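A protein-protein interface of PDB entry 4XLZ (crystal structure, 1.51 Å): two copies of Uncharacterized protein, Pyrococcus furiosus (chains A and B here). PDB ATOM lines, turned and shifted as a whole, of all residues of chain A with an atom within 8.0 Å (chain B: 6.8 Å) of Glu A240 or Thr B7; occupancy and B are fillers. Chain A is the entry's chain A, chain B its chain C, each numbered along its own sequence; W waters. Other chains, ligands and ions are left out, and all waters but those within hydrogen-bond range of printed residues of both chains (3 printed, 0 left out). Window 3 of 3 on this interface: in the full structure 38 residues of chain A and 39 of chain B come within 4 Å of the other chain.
N of Phe B8 lies within hydrogen-bond range of OE2 of Glu A240 (2.7 Å).
The side-chain hydroxyl (OG1) of Thr B7 lies within hydrogen-bond range of the backbone NH (N) of Glu B10. The backbone NH of Ser B6 sits at hydrogen-bond distance from the side-chain carboxylate of Glu B10 (2.9 Å).
Phe B8 touches Thr A233 (CD1 to O, 3.7 Å). Ala B11 touches Thr A233 (CB to OG1, 3.6 Å). Thr A233 touches Phe B12 (CG2 to N, 3.8 Å). CE of Met A236 touches O of Val B5, at 3.8 Å. CE of Met A236 touches C of Ser B6, at 3.7 Å. Thr B7 touches Met A236. Met A236 touches Ala B11. CD1 of Phe B8 touches CA of Phe A237, 3.6 Å away. Glu A240 touches Thr B7 (OE2 to CA, 3.4 Å).
Of chain B, only Thr B7 (3.4 Å) and Phe B8 (2.7 Å) come within 4 Å of Glu A240. Of chain A, only Met A236 (3.5 Å) and Glu A240 (3.4 Å) come within 4 Å of Thr B7. Printed residues of chain A within 4 Å of Phe B8: Thr A233 (3.7 Å), Phe A237 (3.6 Å) and Glu A240 (2.7 Å). Of the printed residues of chain B, Met A236 touches Val B5, Ser B6, Thr B7 and Ala B11. Of the printed residues of chain A, Phe B12 touches Thr A233 (3.8 Å). Printed residues of chain B within 4 Å of Thr A233: Phe B8 (3.7 Å), Ala B11 (3.6 Å) and Phe B12 (3.8 Å). Printed residues of chain B within 4 Å of Phe A237: Phe B8 (3.6 Å). The nearest residue of chain A that does not touch Thr B7 is Thr A233 (6.8 Å). The nearest printed residue of chain B that does not touch Thr A233 is Val B5 (6.2 Å).
Of the 17 printed residues of chain A, 4 touch a printed residue of chain B. Among the printed residues, no Asp or Glu carboxylate lies within 4 Å of a Lys or Arg side-chain nitrogen of the other chain.
No position is printed for both chains.
Water W1 bridges OE1 of Glu A240 (2.5 Å) and N of Glu B9 (2.9 Å). Water W2 bridges NE of Arg A245 and O of Val B5. Water W3 bridges OE2 of Glu A240 and O of Ser B6.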
ATOM      1  N   ILE A 198      -2.988 -14.420 -15.315  1.00  0.00           N
ATOM      2  CA  ILE A 198      -3.074 -13.641 -14.067  1.00  0.00           C
ATOM      3  C   ILE A 198      -2.762 -12.162 -14.378  1.00  0.00           C
ATOM      4  O   ILE A 198      -1.820 -11.874 -15.164  1.00  0.00           O
ATOM      5  CB  ILE A 198      -1.949 -14.048 -13.067  1.00  0.00           C
ATOM      6  CG1 ILE A 198      -1.860 -15.517 -12.888  1.00  0.00           C
ATOM      7  CG2 ILE A 198      -2.035 -13.199 -11.759  1.00  0.00           C
ATOM      8  CD1 ILE A 198      -3.105 -16.046 -12.225  1.00  0.00           C
ATOM      9  N   ARG A 232      -6.482 -10.530   0.880  1.00  0.00           N
ATOM     10  CA  ARG A 232      -5.106 -10.514   0.558  1.00  0.00           C
ATOM     11  C   ARG A 232      -4.446 -11.863   0.363  1.00  0.00           C
ATOM     12  O   ARG A 232      -3.559 -11.946  -0.481  1.00  0.00           O
ATOM     13  CB  ARG A 232      -4.318  -9.790   1.744  1.00  0.00           C
ATOM     14  CG  ARG A 232      -4.827  -8.405   2.014  1.00  0.00           C
ATOM     15  CD  ARG A 232      -3.616  -7.451   2.268  1.00  0.00           C
ATOM     16  NE  ARG A 232      -4.126  -6.113   2.639  1.00  0.00           N
ATOM     17  CZ  ARG A 232      -3.842  -5.027   1.919  1.00  0.00           C
ATOM     18  NH1 ARG A 232      -2.953  -5.060   0.911  1.00  0.00           N
ATOM     19  NH2 ARG A 232      -4.374  -3.850   2.360  1.00  0.00           N
ATOM     20  N   THR A 233      -4.966 -12.882   1.091  1.00  0.00           N
ATOM     21  CA  THR A 233      -4.417 -14.226   0.902  1.00  0.00           C
ATOM     22  C   THR A 233      -4.762 -14.764  -0.546  1.00  0.00           C
ATOM     23  O   THR A 233      -3.893 -15.286  -1.266  1.00  0.00           O
ATOM     24  CB  THR A 233      -4.918 -15.171   1.918  1.00  0.00           C
ATOM     25  OG1 THR A 233      -4.529 -14.673   3.235  1.00  0.00           O
ATOM     26  CG2 THR A 233      -4.330 -16.589   1.796  1.00  0.00           C
ATOM     27  N   VAL A 234      -6.030 -14.458  -0.963  1.00  0.00           N
ATOM     28  CA  VAL A 234      -6.396 -14.850  -2.361  1.00  0.00           C
ATOM     29  C   VAL A 234      -5.572 -14.111  -3.410  1.00  0.00           C
ATOM     30  O   VAL A 234      -5.096 -14.707  -4.379  1.00  0.00           O
ATOM     31  CB  VAL A 234      -7.919 -14.655  -2.538  1.00  0.00           C
ATOM     32  CG1 VAL A 234      -8.320 -14.899  -3.965  1.00  0.00           C
ATOM     33  CG2 VAL A 234      -8.693 -15.623  -1.647  1.00  0.00           C
ATOM     34  N   THR A 235      -5.406 -12.802  -3.253  1.00  0.00           N
ATOM     35  CA  THR A 235      -4.581 -12.077  -4.285  1.00  0.00           C
ATOM     36  C   THR A 235      -3.118 -12.495  -4.307  1.00  0.00           C
ATOM     37  O   THR A 235      -2.496 -12.420  -5.333  1.00  0.00           O
ATOM     38  CB  THR A 235      -4.743 -10.538  -4.155  1.00  0.00           C
ATOM     39  OG1 THR A 235      -4.438 -10.180  -2.840  1.00  0.00           O
ATOM     40  CG2 THR A 235      -6.303 -10.297  -4.160  1.00  0.00           C
ATOM     41  N   MET A 236      -2.617 -12.909  -3.116  1.00  0.00           N
ATOM     42  CA  MET A 236      -1.265 -13.480  -3.090  1.00  0.00           C
ATOM     43  C   MET A 236      -1.181 -14.810  -3.774  1.00  0.00           C
ATOM     44  O   MET A 236      -0.229 -15.122  -4.435  1.00  0.00           O
ATOM     45  CB  MET A 236      -0.704 -13.521  -1.677  1.00  0.00           C
ATOM     46  CG  MET A 236      -0.641 -12.093  -1.117  1.00  0.00           C
ATOM     47  SD  MET A 236      -0.110 -12.154   0.823  1.00  0.00           S
ATOM     48  CE  MET A 236       1.642 -12.743   0.451  1.00  0.00           C
ATOM     49  N   PHE A 237      -2.210 -15.630  -3.572  1.00  0.00           N
ATOM     50  CA  PHE A 237      -2.275 -16.928  -4.243  1.00  0.00           C
ATOM     51  C   PHE A 237      -2.108 -16.730  -5.760  1.00  0.00           C
ATOM     52  O   PHE A 237      -1.331 -17.443  -6.361  1.00  0.00           O
ATOM     53  CB  PHE A 237      -3.671 -17.569  -3.894  1.00  0.00           C
ATOM     54  CG  PHE A 237      -4.005 -18.831  -4.664  1.00  0.00           C
ATOM     55  CD1 PHE A 237      -4.884 -18.785  -5.769  1.00  0.00           C
ATOM     56  CD2 PHE A 237      -3.425 -20.036  -4.283  1.00  0.00           C
ATOM     57  CE1 PHE A 237      -5.172 -19.983  -6.501  1.00  0.00           C
ATOM     58  CE2 PHE A 237      -3.792 -21.252  -4.951  1.00  0.00           C
ATOM     59  CZ  PHE A 237      -4.673 -21.207  -6.060  1.00  0.00           C
ATOM     60  N   TYR A 238      -2.859 -15.775  -6.318  1.00  0.00           N
ATOM     61  CA  TYR A 238      -2.735 -15.545  -7.763  1.00  0.00           C
ATOM     62  C   TYR A 238      -1.424 -14.836  -8.158  1.00  0.00           C
ATOM     63  O   TYR A 238      -0.748 -15.225  -9.118  1.00  0.00           O
ATOM     64  CB  TYR A 238      -3.937 -14.679  -8.225  1.00  0.00           C
ATOM     65  CG  TYR A 238      -5.282 -15.446  -8.154  1.00  0.00           C
ATOM     66  CD1 TYR A 238      -5.409 -16.641  -8.842  1.00  0.00           C
ATOM     67  CD2 TYR A 238      -6.340 -14.903  -7.463  1.00  0.00           C
ATOM     68  CE1 TYR A 238      -6.666 -17.350  -8.718  1.00  0.00           C
ATOM     69  CE2 TYR A 238      -7.542 -15.553  -7.353  1.00  0.00           C
ATOM     70  CZ  TYR A 238      -7.676 -16.759  -8.054  1.00  0.00           C
ATOM     71  OH  TYR A 238      -8.937 -17.442  -7.953  1.00  0.00           O
ATOM     72  N   GLY A 239      -1.086 -13.787  -7.374  1.00  0.00           N
ATOM     73  CA  GLY A 239       0.087 -13.005  -7.814  1.00  0.00           C
ATOM     74  C   GLY A 239       1.375 -13.872  -7.738  1.00  0.00           C
ATOM     75  O   GLY A 239       2.233 -13.716  -8.636  1.00  0.00           O
ATOM     76  N   GLU A 240       1.483 -14.757  -6.744  1.00  0.00           N
ATOM     77  CA  GLU A 240       2.714 -15.608  -6.612  1.00  0.00           C
ATOM     78  C   GLU A 240       2.948 -16.472  -7.855  1.00  0.00           C
ATOM     79  O   GLU A 240       4.087 -16.734  -8.273  1.00  0.00           O
ATOM     80  CB  GLU A 240       2.620 -16.397  -5.372  1.00  0.00           C
ATOM     81  CG  GLU A 240       3.954 -17.002  -4.954  1.00  0.00           C
ATOM     82  CD  GLU A 240       3.901 -17.531  -3.528  1.00  0.00           C
ATOM     83  OE1 GLU A 240       3.821 -18.752  -3.323  1.00  0.00           O
ATOM     84  OE2 GLU A 240       3.870 -16.667  -2.607  1.00  0.00           O
ATOM     85  N   LYS A 241       1.870 -16.785  -8.599  1.00  0.00           N
ATOM     86  CA  LYS A 241       1.992 -17.622  -9.811  1.00  0.00           C
ATOM     87  C   LYS A 241       2.731 -16.898 -10.946  1.00  0.00           C
ATOM     88  O   LYS A 241       3.182 -17.549 -11.862  1.00  0.00           O
ATOM     89  CB  LYS A 241       0.583 -18.038 -10.298  1.00  0.00           C
ATOM     90  CG  LYS A 241      -0.056 -19.009  -9.326  1.00  0.00           C
ATOM     91  CD  LYS A 241      -1.511 -19.466  -9.908  1.00  0.00           C
ATOM     92  CE  LYS A 241      -2.203 -20.239  -8.728  1.00  0.00           C
ATOM     93  NZ  LYS A 241      -1.386 -21.297  -8.017  1.00  0.00           N
ATOM     94  N   ILE A 242       2.779 -15.573 -10.932  1.00  0.00           N
ATOM     95  CA  ILE A 242       3.526 -14.825 -11.933  1.00  0.00           C
ATOM     96  C   ILE A 242       4.629 -13.914 -11.256  1.00  0.00           C
ATOM     97  O   ILE A 242       5.140 -12.936 -11.904  1.00  0.00           O
ATOM     98  CB  ILE A 242       2.621 -13.967 -12.885  1.00  0.00           C
ATOM     99  CG1 ILE A 242       1.762 -12.927 -12.097  1.00  0.00           C
ATOM    100  CG2 ILE A 242       1.796 -14.946 -13.785  1.00  0.00           C
ATOM    101  CD1 ILE A 242       1.163 -11.774 -12.956  1.00  0.00           C
ATOM    102  N   GLY A 243       4.914 -14.253 -10.021  1.00  0.00           N
ATOM    103  CA  GLY A 243       6.030 -13.472  -9.291  1.00  0.00           C
ATOM    104  C   GLY A 243       5.732 -11.995  -8.960  1.00  0.00           C
ATOM    105  O   GLY A 243       6.679 -11.155  -8.895  1.00  0.00           O
ATOM    106  N   VAL A 244       4.439 -11.639  -8.756  1.00  0.00           N
ATOM    107  CA  VAL A 244       4.018 -10.321  -8.304  1.00  0.00           C
ATOM    108  C   VAL A 244       3.305 -10.465  -6.973  1.00  0.00           C
ATOM    109  O   VAL A 244       2.929 -11.548  -6.514  1.00  0.00           O
ATOM    110  CB  VAL A 244       3.159  -9.519  -9.389  1.00  0.00           C
ATOM    111  CG1 VAL A 244       3.791  -9.457 -10.722  1.00  0.00           C
ATOM    112  CG2 VAL A 244       1.694 -10.145  -9.445  1.00  0.00           C
ATOM    113  N   ARG A 245       3.209  -9.336  -6.247  1.00  0.00           N
ATOM    114  CA  ARG A 245       2.628  -9.378  -4.897  1.00  0.00           C
ATOM    115  C   ARG A 245       1.098  -9.796  -4.965  1.00  0.00           C
ATOM    116  O   ARG A 245       0.747 -10.662  -4.226  1.00  0.00           O
ATOM    117  CB  ARG A 245       2.754  -8.015  -4.199  1.00  0.00           C
ATOM    118  CG  ARG A 245       2.483  -8.117  -2.751  1.00  0.00           C
ATOM    119  CD  ARG A 245       2.630  -6.743  -2.083  1.00  0.00           C
ATOM    120  NE  ARG A 245       2.479  -6.909  -0.652  1.00  0.00           N
ATOM    121  CZ  ARG A 245       2.245  -5.872   0.230  1.00  0.00           C
ATOM    122  NH1 ARG A 245       2.149  -6.147   1.542  1.00  0.00           N
ATOM    123  NH2 ARG A 245       2.050  -4.579  -0.140  1.00  0.00           N
ATOM    124  N   TYR A 246       0.344  -9.043  -5.755  1.00  0.00           N
ATOM    125  CA  TYR A 246      -1.136  -9.249  -5.767  1.00  0.00           C
ATOM    126  C   TYR A 246      -1.543  -9.431  -7.220  1.00  0.00           C
ATOM    127  O   TYR A 246      -1.248  -8.631  -8.105  1.00  0.00           O
ATOM    128  CB  TYR A 246      -1.834  -7.997  -5.200  1.00  0.00           C
ATOM    129  CG  TYR A 246      -1.480  -7.722  -3.754  1.00  0.00           C
ATOM    130  CD1 TYR A 246      -1.502  -8.759  -2.807  1.00  0.00           C
ATOM    131  CD2 TYR A 246      -1.290  -6.406  -3.381  1.00  0.00           C
ATOM    132  CE1 TYR A 246      -1.254  -8.449  -1.406  1.00  0.00           C
ATOM    133  CE2 TYR A 246      -1.043  -6.094  -2.024  1.00  0.00           C
ATOM    134  CZ  TYR A 246      -1.023  -7.092  -1.079  1.00  0.00           C
ATOM    135  OH  TYR A 246      -0.811  -6.941   0.278  1.00  0.00           O
ATOM    136  N   GLY A 247      -2.330 -10.519  -7.424  1.00  0.00           N
ATOM    137  CA  GLY A 247      -2.853 -10.794  -8.787  1.00  0.00           C
ATOM    138  C   GLY A 247      -4.347 -11.182  -8.695  1.00  0.00           C
ATOM    139  O   GLY A 247      -4.896 -11.486  -7.670  1.00  0.00           O
ATOM    140  N   ASN B   4       2.121  -7.757   6.146  1.00  0.00           N
ATOM    141  CA  ASN B   4       3.489  -8.102   6.501  1.00  0.00           C
ATOM    142  C   ASN B   4       3.886  -9.505   6.162  1.00  0.00           C
ATOM    143  O   ASN B   4       5.062  -9.817   6.082  1.00  0.00           O
ATOM    144  CB  ASN B   4       3.782  -7.641   7.941  1.00  0.00           C
ATOM    145  CG  ASN B   4       3.942  -6.089   7.995  1.00  0.00           C
ATOM    146  OD1 ASN B   4       3.937  -5.410   6.940  1.00  0.00           O
ATOM    147  ND2 ASN B   4       3.928  -5.530   9.163  1.00  0.00           N
ATOM    148  N   VAL B   5       2.980 -10.321   5.712  1.00  0.00           N
ATOM    149  CA  VAL B   5       3.389 -11.634   5.158  1.00  0.00           C
ATOM    150  C   VAL B   5       3.919 -11.495   3.736  1.00  0.00           C
ATOM    151  O   VAL B   5       3.495 -10.562   2.961  1.00  0.00           O
ATOM    152  CB  VAL B   5       2.153 -12.653   5.184  1.00  0.00           C
ATOM    153  CG1 VAL B   5       1.780 -12.939   6.578  1.00  0.00           C
ATOM    154  CG2 VAL B   5       0.888 -11.942   4.537  1.00  0.00           C
ATOM    155  N   SER B   6       4.793 -12.413   3.382  1.00  0.00           N
ATOM    156  CA  SER B   6       5.543 -12.273   2.159  1.00  0.00           C
ATOM    157  C   SER B   6       5.268 -13.306   1.094  1.00  0.00           C
ATOM    158  O   SER B   6       5.677 -13.087  -0.068  1.00  0.00           O
ATOM    159  CB  SER B   6       7.102 -12.441   2.535  1.00  0.00           C
ATOM    160  OG  SER B   6       7.398 -11.084   2.787  1.00  0.00           O
ATOM    161  N   THR B   7       4.744 -14.431   1.556  1.00  0.00           N
ATOM    162  CA  THR B   7       4.465 -15.487   0.557  1.00  0.00           C
ATOM    163  C   THR B   7       3.032 -15.985   0.809  1.00  0.00           C
ATOM    164  O   THR B   7       2.435 -15.885   1.909  1.00  0.00           O
ATOM    165  CB  THR B   7       5.388 -16.739   0.753  1.00  0.00           C
ATOM    166  OG1 THR B   7       5.178 -17.320   2.027  1.00  0.00           O
ATOM    167  CG2 THR B   7       6.910 -16.360   0.618  1.00  0.00           C
ATOM    168  N   PHE B   8       2.514 -16.649  -0.246  1.00  0.00           N
ATOM    169  CA  PHE B   8       1.145 -17.205  -0.085  1.00  0.00           C
ATOM    170  C   PHE B   8       1.143 -18.245   0.993  1.00  0.00           C
ATOM    171  O   PHE B   8       0.245 -18.328   1.827  1.00  0.00           O
ATOM    172  CB  PHE B   8       0.711 -17.858  -1.438  1.00  0.00           C
ATOM    173  CG  PHE B   8      -0.484 -18.747  -1.231  1.00  0.00           C
ATOM    174  CD1 PHE B   8      -1.736 -18.212  -0.915  1.00  0.00           C
ATOM    175  CD2 PHE B   8      -0.338 -20.159  -1.281  1.00  0.00           C
ATOM    176  CE1 PHE B   8      -2.805 -19.083  -0.593  1.00  0.00           C
ATOM    177  CE2 PHE B   8      -1.403 -20.997  -0.942  1.00  0.00           C
ATOM    178  CZ  PHE B   8      -2.662 -20.456  -0.635  1.00  0.00           C
ATOM    179  N   GLU B   9       2.234 -19.052   1.137  1.00  0.00           N
ATOM    180  CA  GLU B   9       2.208 -20.108   2.136  1.00  0.00           C
ATOM    181  C   GLU B   9       2.093 -19.486   3.552  1.00  0.00           C
ATOM    182  O   GLU B   9       1.345 -19.915   4.451  1.00  0.00           O
ATOM    183  CB  GLU B   9       3.518 -20.927   1.970  1.00  0.00           C
ATOM    184  CG  GLU B   9       3.572 -21.993   3.077  1.00  0.00           C
ATOM    185  CD  GLU B   9       4.741 -23.003   2.877  1.00  0.00           C
ATOM    186  OE1 GLU B   9       5.232 -23.084   1.747  1.00  0.00           O
ATOM    187  OE2 GLU B   9       5.149 -23.669   3.861  1.00  0.00           O
ATOM    188  N   GLU B  10       2.880 -18.403   3.708  1.00  0.00           N
ATOM    189  CA  GLU B  10       2.757 -17.692   4.998  1.00  0.00           C
ATOM    190  C   GLU B  10       1.346 -17.119   5.334  1.00  0.00           C
ATOM    191  O   GLU B  10       0.857 -17.232   6.449  1.00  0.00           O
ATOM    192  CB  GLU B  10       3.865 -16.582   4.975  1.00  0.00           C
ATOM    193  CG  GLU B  10       3.959 -15.927   6.251  1.00  0.00           C
ATOM    194  CD  GLU B  10       4.988 -14.771   6.272  1.00  0.00           C
ATOM    195  OE1 GLU B  10       5.643 -14.411   5.257  1.00  0.00           O
ATOM    196  OE2 GLU B  10       5.145 -14.240   7.414  1.00  0.00           O
ATOM    197  N   ALA B  11       0.767 -16.508   4.273  1.00  0.00           N
ATOM    198  CA  ALA B  11      -0.537 -15.969   4.414  1.00  0.00           C
ATOM    199  C   ALA B  11      -1.599 -17.051   4.737  1.00  0.00           C
ATOM    200  O   ALA B  11      -2.481 -16.892   5.589  1.00  0.00           O
ATOM    201  CB  ALA B  11      -0.956 -15.209   3.115  1.00  0.00           C
ATOM    202  N   PHE B  12      -1.523 -18.122   3.938  1.00  0.00           N
ATOM    203  CA  PHE B  12      -2.385 -19.248   4.179  1.00  0.00           C
ATOM    204  C   PHE B  12      -2.346 -19.833   5.596  1.00  0.00           C
ATOM    205  O   PHE B  12      -3.376 -20.025   6.242  1.00  0.00           O
ATOM    206  CB  PHE B  12      -2.094 -20.311   3.070  1.00  0.00           C
ATOM    207  CG  PHE B  12      -2.840 -21.611   3.254  1.00  0.00           C
ATOM    208  CD1 PHE B  12      -4.122 -21.744   2.656  1.00  0.00           C
ATOM    209  CD2 PHE B  12      -2.277 -22.645   3.918  1.00  0.00           C
ATOM    210  CE1 PHE B  12      -4.798 -22.997   2.834  1.00  0.00           C
ATOM    211  CE2 PHE B  12      -2.926 -23.921   4.038  1.00  0.00           C
ATOM    212  CZ  PHE B  12      -4.194 -24.074   3.469  1.00  0.00           C
HETATM  213  O   HOH W   1       4.097 -19.708  -1.049  1.00  0.00           O
HETATM  214  O   HOH W   2       3.024  -9.022   0.623  1.00  0.00           O
HETATM  215  O   HOH W   3       4.351 -14.024  -2.987  1.00  0.00           O
